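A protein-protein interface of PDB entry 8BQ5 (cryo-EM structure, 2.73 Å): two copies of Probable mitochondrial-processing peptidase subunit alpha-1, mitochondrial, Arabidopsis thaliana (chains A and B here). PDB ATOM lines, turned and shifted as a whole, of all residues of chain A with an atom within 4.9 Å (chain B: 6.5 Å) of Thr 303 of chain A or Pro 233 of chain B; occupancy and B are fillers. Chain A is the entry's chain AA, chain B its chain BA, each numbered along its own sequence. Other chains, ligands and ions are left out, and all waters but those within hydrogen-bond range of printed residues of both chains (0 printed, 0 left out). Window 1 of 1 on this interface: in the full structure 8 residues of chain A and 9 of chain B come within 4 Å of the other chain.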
ATOM      1  N   GLN A 301       4.305 -32.382 -12.907  1.00  0.00           N
ATOM      2  CA  GLN A 301       5.777 -32.321 -12.728  1.00  0.00           C
ATOM      3  C   GLN A 301       6.191 -30.860 -12.900  1.00  0.00           C
ATOM      4  O   GLN A 301       6.535 -30.474 -14.036  1.00  0.00           O
ATOM      5  CB  GLN A 301       6.503 -33.238 -13.710  1.00  0.00           C
ATOM      6  CG  GLN A 301       6.226 -34.725 -13.511  1.00  0.00           C
ATOM      7  CD  GLN A 301       6.717 -35.307 -12.207  1.00  0.00           C
ATOM      8  OE1 GLN A 301       5.956 -35.488 -11.259  1.00  0.00           O
ATOM      9  NE2 GLN A 301       7.998 -35.638 -12.162  1.00  0.00           N
ATOM     10  N   HIS A 302       6.149 -30.083 -11.815  1.00  0.00           N
ATOM     11  CA  HIS A 302       6.486 -28.664 -11.858  1.00  0.00           C
ATOM     12  C   HIS A 302       7.958 -28.524 -12.216  1.00  0.00           C
ATOM     13  O   HIS A 302       8.842 -28.818 -11.407  1.00  0.00           O
ATOM     14  CB  HIS A 302       6.172 -27.990 -10.526  1.00  0.00           C
ATOM     15  CG  HIS A 302       6.237 -26.495 -10.577  1.00  0.00           C
ATOM     16  ND1 HIS A 302       7.347 -25.813 -11.023  1.00  0.00           N
ATOM     17  CD2 HIS A 302       5.323 -25.552 -10.248  1.00  0.00           C
ATOM     18  CE1 HIS A 302       7.118 -24.514 -10.961  1.00  0.00           C
ATOM     19  NE2 HIS A 302       5.896 -24.328 -10.496  1.00  0.00           N
ATOM     20  N   THR A 303       8.220 -28.083 -13.444  1.00  0.00           N
ATOM     21  CA  THR A 303       9.554 -27.680 -13.860  1.00  0.00           C
ATOM     22  C   THR A 303       9.731 -26.168 -13.844  1.00  0.00           C
ATOM     23  O   THR A 303      10.821 -25.688 -13.517  1.00  0.00           O
ATOM     24  CB  THR A 303       9.858 -28.217 -15.265  1.00  0.00           C
ATOM     25  OG1 THR A 303       9.649 -29.633 -15.291  1.00  0.00           O
ATOM     26  CG2 THR A 303      11.299 -27.924 -15.652  1.00  0.00           C
ATOM     27  N   GLY A 304       8.682 -25.416 -14.170  1.00  0.00           N
ATOM     28  CA  GLY A 304       8.717 -23.973 -14.089  1.00  0.00           C
ATOM     29  C   GLY A 304       9.268 -23.318 -15.342  1.00  0.00           C
ATOM     30  O   GLY A 304       9.530 -23.952 -16.366  1.00  0.00           O
ATOM     31  N   GLY A 305       9.442 -22.003 -15.245  1.00  0.00           N
ATOM     32  CA  GLY A 305      10.028 -21.214 -16.310  1.00  0.00           C
ATOM     33  C   GLY A 305       9.045 -20.615 -17.298  1.00  0.00           C
ATOM     34  O   GLY A 305       8.784 -19.409 -17.249  1.00  0.00           O
ATOM     35  N   PHE A 486       2.544 -30.356 -17.564  1.00  0.00           N
ATOM     36  CA  PHE A 486       4.002 -30.387 -17.585  1.00  0.00           C
ATOM     37  C   PHE A 486       4.497 -28.977 -17.861  1.00  0.00           C
ATOM     38  O   PHE A 486       3.995 -28.311 -18.771  1.00  0.00           O
ATOM     39  CB  PHE A 486       4.509 -31.383 -18.641  1.00  0.00           C
ATOM     40  CG  PHE A 486       5.977 -31.261 -18.963  1.00  0.00           C
ATOM     41  CD1 PHE A 486       6.870 -32.219 -18.515  1.00  0.00           C
ATOM     42  CD2 PHE A 486       6.458 -30.234 -19.767  1.00  0.00           C
ATOM     43  CE1 PHE A 486       8.215 -32.126 -18.814  1.00  0.00           C
ATOM     44  CE2 PHE A 486       7.797 -30.135 -20.064  1.00  0.00           C
ATOM     45  CZ  PHE A 486       8.678 -31.084 -19.592  1.00  0.00           C
ATOM     46  N   GLY A 487       5.495 -28.537 -17.099  1.00  0.00           N
ATOM     47  CA  GLY A 487       6.023 -27.196 -17.242  1.00  0.00           C
ATOM     48  C   GLY A 487       5.853 -26.376 -15.981  1.00  0.00           C
ATOM     49  O   GLY A 487       6.322 -26.770 -14.910  1.00  0.00           O
ATOM     50  N   HIS B 117      10.040 -16.019  -7.379  1.00  0.00           N
ATOM     51  CA  HIS B 117      10.187 -17.377  -6.872  1.00  0.00           C
ATOM     52  C   HIS B 117      11.655 -17.686  -6.612  1.00  0.00           C
ATOM     53  O   HIS B 117      12.509 -17.466  -7.476  1.00  0.00           O
ATOM     54  CB  HIS B 117       9.593 -18.371  -7.867  1.00  0.00           C
ATOM     55  CG  HIS B 117       8.099 -18.450  -7.821  1.00  0.00           C
ATOM     56  ND1 HIS B 117       7.327 -18.626  -8.949  1.00  0.00           N
ATOM     57  CD2 HIS B 117       7.234 -18.374  -6.782  1.00  0.00           C
ATOM     58  CE1 HIS B 117       6.052 -18.654  -8.607  1.00  0.00           C
ATOM     59  NE2 HIS B 117       5.968 -18.505  -7.297  1.00  0.00           N
ATOM     60  N   GLY B 118      11.945 -18.213  -5.422  1.00  0.00           N
ATOM     61  CA  GLY B 118      13.295 -18.549  -5.029  1.00  0.00           C
ATOM     62  C   GLY B 118      14.047 -17.463  -4.296  1.00  0.00           C
ATOM     63  O   GLY B 118      15.177 -17.708  -3.856  1.00  0.00           O
ATOM     64  N   ILE B 202      19.735 -28.127  -3.817  1.00  0.00           N
ATOM     65  CA  ILE B 202      18.453 -28.588  -4.342  1.00  0.00           C
ATOM     66  C   ILE B 202      18.569 -30.024  -4.837  1.00  0.00           C
ATOM     67  O   ILE B 202      17.668 -30.846  -4.626  1.00  0.00           O
ATOM     68  CB  ILE B 202      17.953 -27.641  -5.449  1.00  0.00           C
ATOM     69  CG1 ILE B 202      17.777 -26.225  -4.894  1.00  0.00           C
ATOM     70  CG2 ILE B 202      16.660 -28.162  -6.060  1.00  0.00           C
ATOM     71  CD1 ILE B 202      16.378 -25.913  -4.416  1.00  0.00           C
ATOM     72  N   PRO B 229       6.794 -23.118  -3.507  1.00  0.00           N
ATOM     73  CA  PRO B 229       7.834 -23.925  -2.860  1.00  0.00           C
ATOM     74  C   PRO B 229       8.895 -23.059  -2.200  1.00  0.00           C
ATOM     75  O   PRO B 229       9.317 -22.034  -2.740  1.00  0.00           O
ATOM     76  CB  PRO B 229       8.420 -24.744  -4.017  1.00  0.00           C
ATOM     77  CG  PRO B 229       8.083 -23.969  -5.245  1.00  0.00           C
ATOM     78  CD  PRO B 229       6.777 -23.292  -4.969  1.00  0.00           C
ATOM     79  N   TYR B 231      11.834 -24.361  -1.763  1.00  0.00           N
ATOM     80  CA  TYR B 231      12.955 -24.761  -2.604  1.00  0.00           C
ATOM     81  C   TYR B 231      12.554 -24.554  -4.060  1.00  0.00           C
ATOM     82  O   TYR B 231      11.789 -25.349  -4.619  1.00  0.00           O
ATOM     83  CB  TYR B 231      13.339 -26.214  -2.338  1.00  0.00           C
ATOM     84  CG  TYR B 231      13.980 -26.445  -0.988  1.00  0.00           C
ATOM     85  CD1 TYR B 231      13.211 -26.498   0.168  1.00  0.00           C
ATOM     86  CD2 TYR B 231      15.351 -26.614  -0.870  1.00  0.00           C
ATOM     87  CE1 TYR B 231      13.792 -26.710   1.403  1.00  0.00           C
ATOM     88  CE2 TYR B 231      15.942 -26.827   0.359  1.00  0.00           C
ATOM     89  CZ  TYR B 231      15.158 -26.875   1.492  1.00  0.00           C
ATOM     90  OH  TYR B 231      15.744 -27.087   2.719  1.00  0.00           O
ATOM     91  N   ALA B 232      13.065 -23.489  -4.668  1.00  0.00           N
ATOM     92  CA  ALA B 232      12.765 -23.161  -6.051  1.00  0.00           C
ATOM     93  C   ALA B 232      13.353 -24.208  -6.994  1.00  0.00           C
ATOM     94  O   ALA B 232      14.366 -24.836  -6.680  1.00  0.00           O
ATOM     95  CB  ALA B 232      13.321 -21.785  -6.399  1.00  0.00           C
ATOM     96  N   PRO B 233      12.739 -24.417  -8.157  1.00  0.00           N
ATOM     97  CA  PRO B 233      13.271 -25.404  -9.096  1.00  0.00           C
ATOM     98  C   PRO B 233      14.430 -24.838  -9.900  1.00  0.00           C
ATOM     99  O   PRO B 233      14.775 -23.659  -9.805  1.00  0.00           O
ATOM    100  CB  PRO B 233      12.066 -25.710  -9.985  1.00  0.00           C
ATOM    101  CG  PRO B 233      11.382 -24.383 -10.087  1.00  0.00           C
ATOM    102  CD  PRO B 233      11.614 -23.671  -8.752  1.00  0.00           C
ATOM    103  N   GLU B 234      15.029 -25.705 -10.715  1.00  0.00           N
ATOM    104  CA  GLU B 234      16.178 -25.305 -11.517  1.00  0.00           C
ATOM    105  C   GLU B 234      15.646 -24.644 -12.793  1.00  0.00           C
ATOM    106  O   GLU B 234      15.958 -25.043 -13.920  1.00  0.00           O
ATOM    107  CB  GLU B 234      17.087 -26.533 -11.743  1.00  0.00           C
ATOM    108  CG  GLU B 234      18.061 -26.540 -12.921  1.00  0.00           C
ATOM    109  CD  GLU B 234      19.316 -25.738 -12.655  1.00  0.00           C
ATOM    110  OE1 GLU B 234      19.455 -24.641 -13.236  1.00  0.00           O
ATOM    111  OE2 GLU B 234      20.165 -26.209 -11.871  1.00  0.00           O
ATOM    112  N   SER B 235      14.739 -23.698 -12.617  1.00  0.00           N
ATOM    113  CA  SER B 235      14.294 -22.808 -13.683  1.00  0.00           C
ATOM    114  C   SER B 235      14.158 -21.362 -13.230  1.00  0.00           C
ATOM    115  O   SER B 235      14.346 -20.448 -14.036  1.00  0.00           O
ATOM    116  CB  SER B 235      12.963 -23.313 -14.242  1.00  0.00           C
ATOM    117  OG  SER B 235      12.185 -23.909 -13.217  1.00  0.00           O
ATOM    118  N   ALA B 236      13.838 -21.137 -11.954  1.00  0.00           N
ATOM    119  CA  ALA B 236      13.757 -19.790 -11.409  1.00  0.00           C
ATOM    120  C   ALA B 236      15.077 -19.333 -10.812  1.00  0.00           C
ATOM    121  O   ALA B 236      15.192 -18.164 -10.431  1.00  0.00           O
ATOM    122  CB  ALA B 236      12.654 -19.712 -10.351  1.00  0.00           C
ATOM    123  N   LEU B 237      16.062 -20.226 -10.712  1.00  0.00           N
ATOM    124  CA  LEU B 237      17.381 -19.834 -10.229  1.00  0.00           C
ATOM    125  C   LEU B 237      18.196 -19.160 -11.323  1.00  0.00           C
ATOM    126  O   LEU B 237      19.025 -18.288 -11.036  1.00  0.00           O
ATOM    127  CB  LEU B 237      18.122 -21.053  -9.680  1.00  0.00           C
ATOM    128  CG  LEU B 237      17.381 -21.873  -8.625  1.00  0.00           C
ATOM    129  CD1 LEU B 237      18.317 -22.876  -7.974  1.00  0.00           C
ATOM    130  CD2 LEU B 237      16.769 -20.956  -7.576  1.00  0.00           C
ATOM    131  N   ASP B 238      17.983 -19.556 -12.580  1.00  0.00           N
ATOM    132  CA  ASP B 238      18.691 -18.922 -13.685  1.00  0.00           C
ATOM    133  C   ASP B 238      18.280 -17.469 -13.867  1.00  0.00           C
ATOM    134  O   ASP B 238      19.104 -16.650 -14.287  1.00  0.00           O
ATOM    135  CB  ASP B 238      18.448 -19.698 -14.979  1.00  0.00           C
ATOM    136  CG  ASP B 238      19.453 -19.356 -16.059  1.00  0.00           C
ATOM    137  OD1 ASP B 238      20.658 -19.615 -15.851  1.00  0.00           O
ATOM    138  OD2 ASP B 238      19.042 -18.828 -17.113  1.00  0.00           O
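O of Thr 303 of chain A sits close to OG of Ser 235 of chain B (2.3 Å).
The backbone NH of Thr 303 of chain A is in hydrogen-bond range of the backbone carbonyl oxygen of Gly 487 of chain A, at 2.7 Å. N of Gly 304 of chain A is in hydrogen-bond range of ND1 of His 302 of chain A (3.4 Å). The backbone carbonyl oxygen (O) of Gln 301 of chain A lies within hydrogen-bond range of the side-chain hydroxyl (OG1) of Thr 303 of chain A (3.5 Å). The backbone carbonyl oxygen of Gly 487 of chain A is in hydrogen-bond range of the backbone NH of Gly 304 of chain A, at 2.8 Å.
Hydrophobic or aromatic side chains of chain B within 4 Å of the printed part of chain A: Pro 233. Along chain B the printed residues that touch a printed residue of chain A span positions 233 to 235. Of the 7 printed residues of chain A, 3 touch a printed residue of chain B. Among the printed residues, 4 pairs touch across the chains. Among the printed residues, no Asp or Glu carboxylate lies within 4 Å of a Lys or Arg side-chain nitrogen of the other chain.
Thr 303 of chain A touches two residues of chain B. Of the printed residues of chain B, Gly 304 of chain A touches Ser 235. Printed residues of chain B within 4 Å of Gly 305 of chain A: Ser 235 (3.9 Å). Pro 233 of chain B touches one residue of chain A. Of the printed residues of chain A, Ser 235 of chain B touches Thr 303 (2.3 Å), Gly 304 (3.6 Å) and Gly 305 (3.9 Å). The nearest residue of chain B that does not touch Thr 303 of chain A is Glu 234 of chain B (5.0 Å). The nearest residue of chain A that does not touch Pro 233 of chain B is His 302 of chain A (4.4 Å).
No position is printed for both chains. Of the 4 pairs that touch across the chains among the printed residues, none has its exchanged pair printed and touching as well.
O of Thr 303 of chain A touches CG of Pro 233 of chain B, 3.7 Å away. CA of Gly 304 of chain A touches OG of Ser 235 of chain B, at 3.6 Å. Gly 305 of chain A touches Ser 235 of chain B.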
